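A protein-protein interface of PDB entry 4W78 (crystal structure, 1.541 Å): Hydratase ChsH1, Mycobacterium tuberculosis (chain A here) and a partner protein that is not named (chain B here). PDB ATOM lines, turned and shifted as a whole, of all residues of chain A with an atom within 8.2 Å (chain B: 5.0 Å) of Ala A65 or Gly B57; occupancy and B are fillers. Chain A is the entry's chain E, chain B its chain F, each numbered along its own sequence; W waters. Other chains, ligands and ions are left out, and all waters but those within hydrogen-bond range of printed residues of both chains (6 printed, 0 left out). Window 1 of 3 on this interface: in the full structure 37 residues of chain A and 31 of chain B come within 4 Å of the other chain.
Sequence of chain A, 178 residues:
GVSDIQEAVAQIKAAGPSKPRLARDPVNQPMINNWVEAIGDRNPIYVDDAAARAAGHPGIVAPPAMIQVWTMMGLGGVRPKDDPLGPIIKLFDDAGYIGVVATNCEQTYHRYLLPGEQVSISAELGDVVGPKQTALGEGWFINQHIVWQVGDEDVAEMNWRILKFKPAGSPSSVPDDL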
ATOM      1  N   TRP A  35     -11.173  11.343  -0.858  1.00  0.00           N
ATOM      2  CA  TRP A  35     -12.460  11.053  -0.253  1.00  0.00           C
ATOM      3  C   TRP A  35     -13.053  12.292   0.399  1.00  0.00           C
ATOM      4  O   TRP A  35     -14.213  12.612   0.172  1.00  0.00           O
ATOM      5  CB  TRP A  35     -12.281   9.917   0.749  1.00  0.00           C
ATOM      6  CG  TRP A  35     -13.520   9.314   1.339  1.00  0.00           C
ATOM      7  CD1 TRP A  35     -14.142   8.179   0.920  1.00  0.00           C
ATOM      8  CD2 TRP A  35     -14.239   9.765   2.497  1.00  0.00           C
ATOM      9  NE1 TRP A  35     -15.204   7.893   1.733  1.00  0.00           N
ATOM     10  CE2 TRP A  35     -15.297   8.855   2.699  1.00  0.00           C
ATOM     11  CE3 TRP A  35     -14.096  10.843   3.369  1.00  0.00           C
ATOM     12  CZ2 TRP A  35     -16.208   8.979   3.744  1.00  0.00           C
ATOM     13  CZ3 TRP A  35     -15.015  10.971   4.417  1.00  0.00           C
ATOM     14  CH2 TRP A  35     -16.062  10.042   4.576  1.00  0.00           C
ATOM     15  N   ILE A  39     -16.626  13.928  -0.804  1.00  0.00           N
ATOM     16  CA  ILE A  39     -17.687  13.897   0.195  1.00  0.00           C
ATOM     17  C   ILE A  39     -17.972  15.309   0.703  1.00  0.00           C
ATOM     18  O   ILE A  39     -19.081  15.602   1.155  1.00  0.00           O
ATOM     19  CB  ILE A  39     -17.281  12.961   1.382  1.00  0.00           C
ATOM     20  CG1 ILE A  39     -17.170  11.510   0.903  1.00  0.00           C
ATOM     21  CG2 ILE A  39     -18.253  13.044   2.573  1.00  0.00           C
ATOM     22  CD1 ILE A  39     -18.508  10.875   0.519  1.00  0.00           C
ATOM     23  N   GLY A  40     -16.970  16.192   0.621  1.00  0.00           N
ATOM     24  CA  GLY A  40     -17.120  17.563   1.078  1.00  0.00           C
ATOM     25  C   GLY A  40     -17.039  17.705   2.594  1.00  0.00           C
ATOM     26  O   GLY A  40     -17.582  18.661   3.151  1.00  0.00           O
ATOM     27  N   ASP A  41     -16.364  16.758   3.243  1.00  0.00           N
ATOM     28  CA  ASP A  41     -16.236  16.761   4.691  1.00  0.00           C
ATOM     29  C   ASP A  41     -14.987  17.553   5.058  1.00  0.00           C
ATOM     30  O   ASP A  41     -13.865  17.097   4.811  1.00  0.00           O
ATOM     31  CB  ASP A  41     -16.140  15.326   5.202  1.00  0.00           C
ATOM     32  CG  ASP A  41     -16.241  15.234   6.713  1.00  0.00           C
ATOM     33  OD1 ASP A  41     -16.037  16.261   7.386  1.00  0.00           O
ATOM     34  OD2 ASP A  41     -16.511  14.122   7.215  1.00  0.00           O
ATOM     35  N   TYR A  46      -8.847  15.048   9.558  1.00  0.00           N
ATOM     36  CA  TYR A  46      -8.481  14.115   8.491  1.00  0.00           C
ATOM     37  C   TYR A  46      -7.381  14.675   7.611  1.00  0.00           C
ATOM     38  O   TYR A  46      -6.850  13.958   6.766  1.00  0.00           O
ATOM     39  CB  TYR A  46      -9.687  13.832   7.594  1.00  0.00           C
ATOM     40  CG  TYR A  46     -10.915  13.330   8.318  1.00  0.00           C
ATOM     41  CD1 TYR A  46     -10.815  12.454   9.393  1.00  0.00           C
ATOM     42  CD2 TYR A  46     -12.185  13.725   7.911  1.00  0.00           C
ATOM     43  CE1 TYR A  46     -11.957  11.998  10.059  1.00  0.00           C
ATOM     44  CE2 TYR A  46     -13.326  13.278   8.575  1.00  0.00           C
ATOM     45  CZ  TYR A  46     -13.202  12.405   9.646  1.00  0.00           C
ATOM     46  OH  TYR A  46     -14.314  11.945  10.309  1.00  0.00           O
ATOM     47  N   ALA A  62      -7.839   8.650   9.799  1.00  0.00           N
ATOM     48  CA  ALA A  62      -8.728   8.416   8.662  1.00  0.00           C
ATOM     49  C   ALA A  62     -10.185   8.554   9.078  1.00  0.00           C
ATOM     50  O   ALA A  62     -10.541   8.216  10.198  1.00  0.00           O
ATOM     51  CB  ALA A  62      -8.485   7.006   8.094  1.00  0.00           C
ATOM     52  N   PRO A  63     -11.045   9.016   8.160  1.00  0.00           N
ATOM     53  CA  PRO A  63     -12.475   9.002   8.472  1.00  0.00           C
ATOM     54  C   PRO A  63     -12.920   7.569   8.741  1.00  0.00           C
ATOM     55  O   PRO A  63     -12.557   6.658   7.979  1.00  0.00           O
ATOM     56  CB  PRO A  63     -13.133   9.552   7.196  1.00  0.00           C
ATOM     57  CG  PRO A  63     -12.034  10.323   6.476  1.00  0.00           C
ATOM     58  CD  PRO A  63     -10.738   9.644   6.863  1.00  0.00           C
ATOM     59  N   PRO A  64     -13.662   7.342   9.833  1.00  0.00           N
ATOM     60  CA  PRO A  64     -14.102   5.974  10.150  1.00  0.00           C
ATOM     61  C   PRO A  64     -14.847   5.317   8.976  1.00  0.00           C
ATOM     62  O   PRO A  64     -14.619   4.143   8.650  1.00  0.00           O
ATOM     63  CB  PRO A  64     -15.029   6.178  11.356  1.00  0.00           C
ATOM     64  CG  PRO A  64     -14.431   7.394  12.037  1.00  0.00           C
ATOM     65  CD  PRO A  64     -13.983   8.300  10.912  1.00  0.00           C
ATOM     66  N   ALA A  65     -15.696   6.097   8.326  1.00  0.00           N
ATOM     67  CA  ALA A  65     -16.508   5.590   7.217  1.00  0.00           C
ATOM     68  C   ALA A  65     -15.710   5.263   5.960  1.00  0.00           C
ATOM     69  O   ALA A  65     -16.276   4.760   4.994  1.00  0.00           O
ATOM     70  CB  ALA A  65     -17.636   6.594   6.901  1.00  0.00           C
ATOM     71  N   MET A  66     -14.411   5.525   5.965  1.00  0.00           N
ATOM     72  CA  MET A  66     -13.560   5.023   4.880  1.00  0.00           C
ATOM     73  C   MET A  66     -13.153   3.558   5.028  1.00  0.00           C
ATOM     74  O   MET A  66     -12.431   3.042   4.175  1.00  0.00           O
ATOM     75  CB  MET A  66     -12.282   5.856   4.746  1.00  0.00           C
ATOM     76  CG  MET A  66     -12.481   7.177   4.029  1.00  0.00           C
ATOM     77  SD  MET A  66     -10.922   7.939   3.576  1.00  0.00           S
ATOM     78  CE  MET A  66     -10.523   6.973   2.110  1.00  0.00           C
ATOM     79  N   ILE A  67     -13.571   2.882   6.101  1.00  0.00           N
ATOM     80  CA  ILE A  67     -13.062   1.527   6.352  1.00  0.00           C
ATOM     81  C   ILE A  67     -13.206   0.589   5.148  1.00  0.00           C
ATOM     82  O   ILE A  67     -12.262  -0.089   4.761  1.00  0.00           O
ATOM     83  CB  ILE A  67     -13.636   0.890   7.657  1.00  0.00           C
ATOM     84  CG1 ILE A  67     -12.938  -0.439   7.971  1.00  0.00           C
ATOM     85  CG2 ILE A  67     -15.148   0.724   7.598  1.00  0.00           C
ATOM     86  CD1 ILE A  67     -11.477  -0.263   8.336  1.00  0.00           C
ATOM     87  N   GLN A  68     -14.382   0.611   4.532  1.00  0.00           N
ATOM     88  CA  GLN A  68     -14.644  -0.286   3.416  1.00  0.00           C
ATOM     89  C   GLN A  68     -13.845   0.128   2.170  1.00  0.00           C
ATOM     90  O   GLN A  68     -13.555  -0.700   1.302  1.00  0.00           O
ATOM     91  CB  GLN A  68     -16.157  -0.317   3.162  1.00  0.00           C
ATOM     92  CG  GLN A  68     -16.686  -1.423   2.279  1.00  0.00           C
ATOM     93  CD  GLN A  68     -18.217  -1.412   2.246  1.00  0.00           C
ATOM     94  OE1 GLN A  68     -18.856  -0.645   2.965  1.00  0.00           O
ATOM     95  NE2 GLN A  68     -18.794  -2.242   1.410  1.00  0.00           N
ATOM     96  N   VAL A  69     -13.481   1.405   2.074  1.00  0.00           N
ATOM     97  CA  VAL A  69     -12.749   1.905   0.922  1.00  0.00           C
ATOM     98  C   VAL A  69     -11.391   1.216   0.767  1.00  0.00           C
ATOM     99  O   VAL A  69     -10.963   0.916  -0.352  1.00  0.00           O
ATOM    100  CB  VAL A  69     -12.579   3.442   1.002  1.00  0.00           C
ATOM    101  CG1 VAL A  69     -11.862   3.969  -0.238  1.00  0.00           C
ATOM    102  CG2 VAL A  69     -13.940   4.118   1.116  1.00  0.00           C
ATOM    103  N   TRP A  70     -10.709   0.966   1.888  1.00  0.00           N
ATOM    104  CA  TRP A  70      -9.347   0.462   1.807  1.00  0.00           C
ATOM    105  C   TRP A  70      -9.279  -0.894   1.137  1.00  0.00           C
ATOM    106  O   TRP A  70      -8.304  -1.210   0.441  1.00  0.00           O
ATOM    107  CB  TRP A  70      -8.691   0.376   3.198  1.00  0.00           C
ATOM    108  CG  TRP A  70      -8.772   1.675   3.950  1.00  0.00           C
ATOM    109  CD1 TRP A  70      -9.486   1.925   5.088  1.00  0.00           C
ATOM    110  CD2 TRP A  70      -8.161   2.910   3.567  1.00  0.00           C
ATOM    111  NE1 TRP A  70      -9.348   3.248   5.453  1.00  0.00           N
ATOM    112  CE2 TRP A  70      -8.543   3.873   4.530  1.00  0.00           C
ATOM    113  CE3 TRP A  70      -7.352   3.301   2.490  1.00  0.00           C
ATOM    114  CZ2 TRP A  70      -8.131   5.194   4.461  1.00  0.00           C
ATOM    115  CZ3 TRP A  70      -6.928   4.640   2.423  1.00  0.00           C
ATOM    116  CH2 TRP A  70      -7.326   5.564   3.416  1.00  0.00           C
ATOM    117  N   CYS A 105     -26.648  -0.924   5.694  1.00  0.00           N
ATOM    118  CA  CYS A 105     -25.254  -1.033   6.083  1.00  0.00           C
ATOM    119  C   CYS A 105     -25.139  -0.629   7.541  1.00  0.00           C
ATOM    120  O   CYS A 105     -25.591   0.446   7.916  1.00  0.00           O
ATOM    121  CB  CYS A 105     -24.387  -0.128   5.208  1.00  0.00           C
ATOM    122  SG  CYS A 105     -22.605  -0.210   5.541  1.00  0.00           S
ATOM    123  N   GLN A 107     -22.095  -0.313  10.412  1.00  0.00           N
ATOM    124  CA  GLN A 107     -20.667  -0.406  10.685  1.00  0.00           C
ATOM    125  C   GLN A 107     -20.380   0.015  12.115  1.00  0.00           C
ATOM    126  O   GLN A 107     -20.974   0.964  12.607  1.00  0.00           O
ATOM    127  CB  GLN A 107     -19.880   0.499   9.736  1.00  0.00           C
ATOM    128  CG  GLN A 107     -20.024   0.108   8.259  1.00  0.00           C
ATOM    129  CD  GLN A 107     -19.122   0.905   7.327  1.00  0.00           C
ATOM    130  OE1 GLN A 107     -18.670   2.009   7.647  1.00  0.00           O
ATOM    131  NE2 GLN A 107     -18.858   0.340   6.152  1.00  0.00           N
ATOM    132  N   TYR A 109     -17.014   0.971  14.661  1.00  0.00           N
ATOM    133  CA  TYR A 109     -15.608   1.337  14.557  1.00  0.00           C
ATOM    134  C   TYR A 109     -14.983   1.235  15.932  1.00  0.00           C
ATOM    135  O   TYR A 109     -15.361   1.967  16.840  1.00  0.00           O
ATOM    136  CB  TYR A 109     -15.460   2.757  13.989  1.00  0.00           C
ATOM    137  CG  TYR A 109     -16.358   3.031  12.805  1.00  0.00           C
ATOM    138  CD1 TYR A 109     -16.109   2.450  11.566  1.00  0.00           C
ATOM    139  CD2 TYR A 109     -17.456   3.877  12.924  1.00  0.00           C
ATOM    140  CE1 TYR A 109     -16.943   2.701  10.484  1.00  0.00           C
ATOM    141  CE2 TYR A 109     -18.290   4.133  11.859  1.00  0.00           C
ATOM    142  CZ  TYR A 109     -18.033   3.539  10.633  1.00  0.00           C
ATOM    143  OH  TYR A 109     -18.884   3.819   9.589  1.00  0.00           O
ATOM    144  N   TYR A 112     -10.147   4.814  15.654  1.00  0.00           N
ATOM    145  CA  TYR A 112      -9.731   5.498  14.436  1.00  0.00           C
ATOM    146  C   TYR A 112      -8.403   4.930  13.947  1.00  0.00           C
ATOM    147  O   TYR A 112      -7.562   4.498  14.748  1.00  0.00           O
ATOM    148  CB  TYR A 112      -9.597   7.013  14.698  1.00  0.00           C
ATOM    149  CG  TYR A 112     -10.923   7.764  14.728  1.00  0.00           C
ATOM    150  CD1 TYR A 112     -11.931   7.412  15.617  1.00  0.00           C
ATOM    151  CD2 TYR A 112     -11.153   8.834  13.884  1.00  0.00           C
ATOM    152  CE1 TYR A 112     -13.147   8.088  15.636  1.00  0.00           C
ATOM    153  CE2 TYR A 112     -12.366   9.522  13.892  1.00  0.00           C
ATOM    154  CZ  TYR A 112     -13.361   9.138  14.763  1.00  0.00           C
ATOM    155  OH  TYR A 112     -14.567   9.801  14.770  1.00  0.00           O
ATOM    156  N   TRP A 148     -12.755  -6.200   9.859  1.00  0.00           N
ATOM    157  CA  TRP A 148     -11.461  -5.648   9.467  1.00  0.00           C
ATOM    158  C   TRP A 148     -10.505  -5.709  10.640  1.00  0.00           C
ATOM    159  O   TRP A 148     -10.898  -5.469  11.788  1.00  0.00           O
ATOM    160  CB  TRP A 148     -11.592  -4.192   9.027  1.00  0.00           C
ATOM    161  CG  TRP A 148     -12.285  -4.000   7.711  1.00  0.00           C
ATOM    162  CD1 TRP A 148     -11.713  -4.043   6.472  1.00  0.00           C
ATOM    163  CD2 TRP A 148     -13.677  -3.721   7.502  1.00  0.00           C
ATOM    164  NE1 TRP A 148     -12.661  -3.805   5.507  1.00  0.00           N
ATOM    165  CE2 TRP A 148     -13.874  -3.604   6.108  1.00  0.00           C
ATOM    166  CE3 TRP A 148     -14.771  -3.543   8.358  1.00  0.00           C
ATOM    167  CZ2 TRP A 148     -15.120  -3.329   5.547  1.00  0.00           C
ATOM    168  CZ3 TRP A 148     -16.016  -3.256   7.792  1.00  0.00           C
ATOM    169  CH2 TRP A 148     -16.172  -3.149   6.404  1.00  0.00           C
ATOM    170  N   LEU B  53     -21.552   3.550   0.179  1.00  0.00           N
ATOM    171  CA  LEU B  53     -20.349   4.014   0.894  1.00  0.00           C
ATOM    172  C   LEU B  53     -20.383   5.533   0.999  1.00  0.00           C
ATOM    173  O   LEU B  53     -19.890   6.105   1.967  1.00  0.00           O
ATOM    174  CB  LEU B  53     -19.041   3.554   0.221  1.00  0.00           C
ATOM    175  CG  LEU B  53     -18.694   2.051   0.296  1.00  0.00           C
ATOM    176  CD1 LEU B  53     -19.562   1.229  -0.649  1.00  0.00           C
ATOM    177  CD2 LEU B  53     -17.229   1.778  -0.018  1.00  0.00           C
ATOM    178  N   THR B  54     -20.944   6.196  -0.004  1.00  0.00           N
ATOM    179  CA  THR B  54     -21.102   7.644   0.051  1.00  0.00           C
ATOM    180  C   THR B  54     -22.206   8.029   1.040  1.00  0.00           C
ATOM    181  O   THR B  54     -22.046   8.987   1.794  1.00  0.00           O
ATOM    182  CB  THR B  54     -21.394   8.216  -1.349  1.00  0.00           C
ATOM    183  OG1 THR B  54     -20.239   8.010  -2.175  1.00  0.00           O
ATOM    184  CG2 THR B  54     -21.736   9.696  -1.283  1.00  0.00           C
ATOM    185  N   ASP B  55     -23.321   7.300   1.056  1.00  0.00           N
ATOM    186  CA  ASP B  55     -24.336   7.535   2.096  1.00  0.00           C
ATOM    187  C   ASP B  55     -23.744   7.460   3.511  1.00  0.00           C
ATOM    188  O   ASP B  55     -24.025   8.316   4.362  1.00  0.00           O
ATOM    189  CB  ASP B  55     -25.498   6.545   1.979  1.00  0.00           C
ATOM    190  CG  ASP B  55     -26.405   6.842   0.806  1.00  0.00           C
ATOM    191  OD1 ASP B  55     -26.682   8.039   0.551  1.00  0.00           O
ATOM    192  OD2 ASP B  55     -26.857   5.879   0.146  1.00  0.00           O
ATOM    193  N   THR B  56     -22.936   6.432   3.766  1.00  0.00           N
ATOM    194  CA  THR B  56     -22.295   6.294   5.074  1.00  0.00           C
ATOM    195  C   THR B  56     -21.379   7.502   5.365  1.00  0.00           C
ATOM    196  O   THR B  56     -21.391   8.068   6.479  1.00  0.00           O
ATOM    197  CB  THR B  56     -21.477   4.999   5.144  1.00  0.00           C
ATOM    198  OG1 THR B  56     -22.325   3.882   4.829  1.00  0.00           O
ATOM    199  CG2 THR B  56     -20.893   4.809   6.540  1.00  0.00           C
ATOM    200  N   GLY B  57     -20.591   7.911   4.375  1.00  0.00           N
ATOM    201  CA  GLY B  57     -19.675   9.028   4.536  1.00  0.00           C
ATOM    202  C   GLY B  57     -20.414  10.328   4.769  1.00  0.00           C
ATOM    203  O   GLY B  57     -19.975  11.155   5.572  1.00  0.00           O
ATOM    204  N   LEU B  58     -21.523  10.524   4.055  1.00  0.00           N
ATOM    205  CA  LEU B  58     -22.318  11.747   4.205  1.00  0.00           C
ATOM    206  C   LEU B  58     -23.007  11.807   5.570  1.00  0.00           C
ATOM    207  O   LEU B  58     -23.074  12.882   6.189  1.00  0.00           O
ATOM    208  CB  LEU B  58     -23.351  11.863   3.085  1.00  0.00           C
ATOM    209  CG  LEU B  58     -22.740  12.140   1.714  1.00  0.00           C
ATOM    210  CD1 LEU B  58     -23.832  12.070   0.652  1.00  0.00           C
ATOM    211  CD2 LEU B  58     -22.051  13.495   1.700  1.00  0.00           C
ATOM    212  N   VAL B  59     -23.531  10.679   6.046  1.00  0.00           N
ATOM    213  CA  VAL B  59     -24.121  10.643   7.391  1.00  0.00           C
ATOM    214  C   VAL B  59     -23.067  11.002   8.444  1.00  0.00           C
ATOM    215  O   VAL B  59     -23.339  11.783   9.382  1.00  0.00           O
ATOM    216  CB  VAL B  59     -24.748   9.263   7.683  1.00  0.00           C
ATOM    217  CG1 VAL B  59     -25.038   9.094   9.165  1.00  0.00           C
ATOM    218  CG2 VAL B  59     -26.018   9.067   6.848  1.00  0.00           C
ATOM    219  N   GLN B  60     -21.868  10.445   8.298  1.00  0.00           N
ATOM    220  CA  GLN B  60     -20.745  10.799   9.168  1.00  0.00           C
ATOM    221  C   GLN B  60     -20.462  12.288   9.134  1.00  0.00           C
ATOM    222  O   GLN B  60     -20.364  12.929  10.196  1.00  0.00           O
ATOM    223  CB  GLN B  60     -19.498  10.023   8.742  1.00  0.00           C
ATOM    224  CG  GLN B  60     -18.310  10.209   9.666  1.00  0.00           C
ATOM    225  CD  GLN B  60     -17.141   9.394   9.203  1.00  0.00           C
ATOM    226  OE1 GLN B  60     -16.903   8.296   9.694  1.00  0.00           O
ATOM    227  NE2 GLN B  60     -16.413   9.919   8.240  1.00  0.00           N
ATOM    228  N   ARG B  61     -20.297  12.839   7.935  1.00  0.00           N
ATOM    229  CA  ARG B  61     -20.019  14.269   7.759  1.00  0.00           C
ATOM    230  C   ARG B  61     -21.100  15.126   8.401  1.00  0.00           C
ATOM    231  O   ARG B  61     -20.807  16.100   9.106  1.00  0.00           O
ATOM    232  CB  ARG B  61     -19.957  14.605   6.274  1.00  0.00           C
ATOM    233  CG  ARG B  61     -19.899  16.097   6.036  1.00  0.00           C
ATOM    234  CD  ARG B  61     -20.119  16.434   4.583  1.00  0.00           C
ATOM    235  NE  ARG B  61     -20.453  17.848   4.466  1.00  0.00           N
ATOM    236  CZ  ARG B  61     -20.765  18.445   3.327  1.00  0.00           C
ATOM    237  NH1 ARG B  61     -20.776  17.748   2.192  1.00  0.00           N
ATOM    238  NH2 ARG B  61     -21.065  19.737   3.323  1.00  0.00           N
ATOM    239  N   ILE B  76     -22.303   3.559  12.716  1.00  0.00           N
ATOM    240  CA  ILE B  76     -23.285   4.147  11.816  1.00  0.00           C
ATOM    241  C   ILE B  76     -24.105   3.006  11.259  1.00  0.00           C
ATOM    242  O   ILE B  76     -23.554   2.080  10.663  1.00  0.00           O
ATOM    243  CB  ILE B  76     -22.622   4.910  10.657  1.00  0.00           C
ATOM    244  CG1 ILE B  76     -21.854   6.133  11.176  1.00  0.00           C
ATOM    245  CG2 ILE B  76     -23.672   5.361   9.619  1.00  0.00           C
ATOM    246  CD1 ILE B  76     -20.982   6.791  10.104  1.00  0.00           C
HETATM  247  O   HOH W   1     -19.967   2.076   3.654  1.00  0.00           O
HETATM  248  O   HOH W   2     -17.317  11.912   6.718  1.00  0.00           O
HETATM  249  O   HOH W   3     -17.094   5.762   2.492  1.00  0.00           O
HETATM  250  O   HOH W   4     -18.027  19.459   6.158  1.00  0.00           O
HETATM  251  O   HOH W   5     -17.516  17.221   9.413  1.00  0.00           O
HETATM  252  O   HOH W   6     -23.085   2.266   7.462  1.00  0.00           O
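The side-chain amide oxygen (OE1) of Gln B60 is in hydrogen-bond range of the backbone NH (N) of Ala A65 (2.9 Å). The backbone carbonyl oxygen of Ile A39 sits at hydrogen-bond distance from the guanidinium group of Arg B61 (2.9 Å). The backbone NH (N) of Gln A107 lies within hydrogen-bond range of the backbone carbonyl oxygen (O) of Ile B76, 2.8 Å away. NE of Arg B61 lies close to O of Gly A40 (3.3 Å). The side-chain amide oxygen (OE1) of Gln B60 lies close to the backbone nitrogen (N) of Pro A64 (3.4 Å).
The side-chain amide nitrogen (NE2) of Gln A107 is in hydrogen-bond range of the side-chain amide oxygen (OE1) of Gln A68. OH of Tyr A109 lies within hydrogen-bond range of OE1 of Gln A107 (2.7 Å).
CA of Gly B57 touches CZ2 of Trp A35, at 3.6 Å. Gln B60 touches Trp A35. Ile A39 touches Leu B58. Asp A41 touches Arg B61 (OD2 to CA, 3.6 Å). Tyr A46 touches Gln B60 (OH to NE2, 3.6 Å). Thr B56 touches Ala A65. Gln A68 touches Leu B53. Cys A105 touches Ile B76 (O to O, 3.8 Å). Gln A107 touches Thr B56 (OE1 to CG2, 3.7 Å). Tyr A109 touches Thr B56.
Printed residues of chain B within 4 Å of Tyr A46: Gln B60 (3.6 Å). Ala A65 touches just these residues of chain B: Thr B56 (3.7 Å), Gly B57 (3.96 Å) and Gln B60 (2.9 Å). Printed residues of chain B within 4 Å of Gln A68: Leu B53. Trp A70 touches none of the printed residues of chain B. Printed residues of chain A within 4 Å of Thr B54: Ile A39. Asp B55 touches none of the printed residues of chain A. Gly B57 touches just these residues of chain A: Trp A35, Ile A39 and Ala A65. Printed residues of chain A within 4 Å of Gln B60: Trp A35, Tyr A46, Pro A63, Pro A64 and Ala A65. Printed residues of chain A within 4 Å of Ile B76: Cys A105 (3.8 Å), Gln A107 (2.8 Å) and Tyr A109 (3.7 Å). The nearest residue of chain A that does not touch Gly B57 is Asp A41 (4.8 Å).
Hydrophobic or aromatic side chains of chain A within 4 Å of the printed part of chain B: Trp A35, Ile A39, Tyr A46, Pro A63, Pro A64, Ala A65 and Tyr A109. Of the 10 printed residues of chain B, 8 touch a printed residue of chain A.
Water W2 lies within hydrogen-bond range of OD2 of Asp A41 (2.4 Å), NE2 of Gln B60 (2.7 Å), O of Gly B57 (3.0 Å) and N of Arg B61 (3.3 Å). Water W5 bridges OD1 of Asp A41 (2.7 Å) and O of Arg B61 (3.5 Å). Water W3 lies within hydrogen-bond range of the backbone carbonyl oxygen (O) of Ala A65, the backbone carbonyl oxygen (O) of Leu B53 and the indole nitrogen (NE1) of Trp A35. Water W1 lies within hydrogen-bond range of the side-chain amide oxygen of Gln A68 (3.0 Å), the side-chain hydroxyl of Thr B56 (3.2 Å) and the side-chain amide nitrogen of Gln A107 (3.2 Å). Water W6 lies within hydrogen-bond range of O of Cys A105 (3.1 Å), OG1 of Thr B56 (3.2 Å) and O of Ile B76 (3.2 Å). Water W4 bridges O of Gly A40 (3.1 Å) and NE of Arg B61 (3.4 Å).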
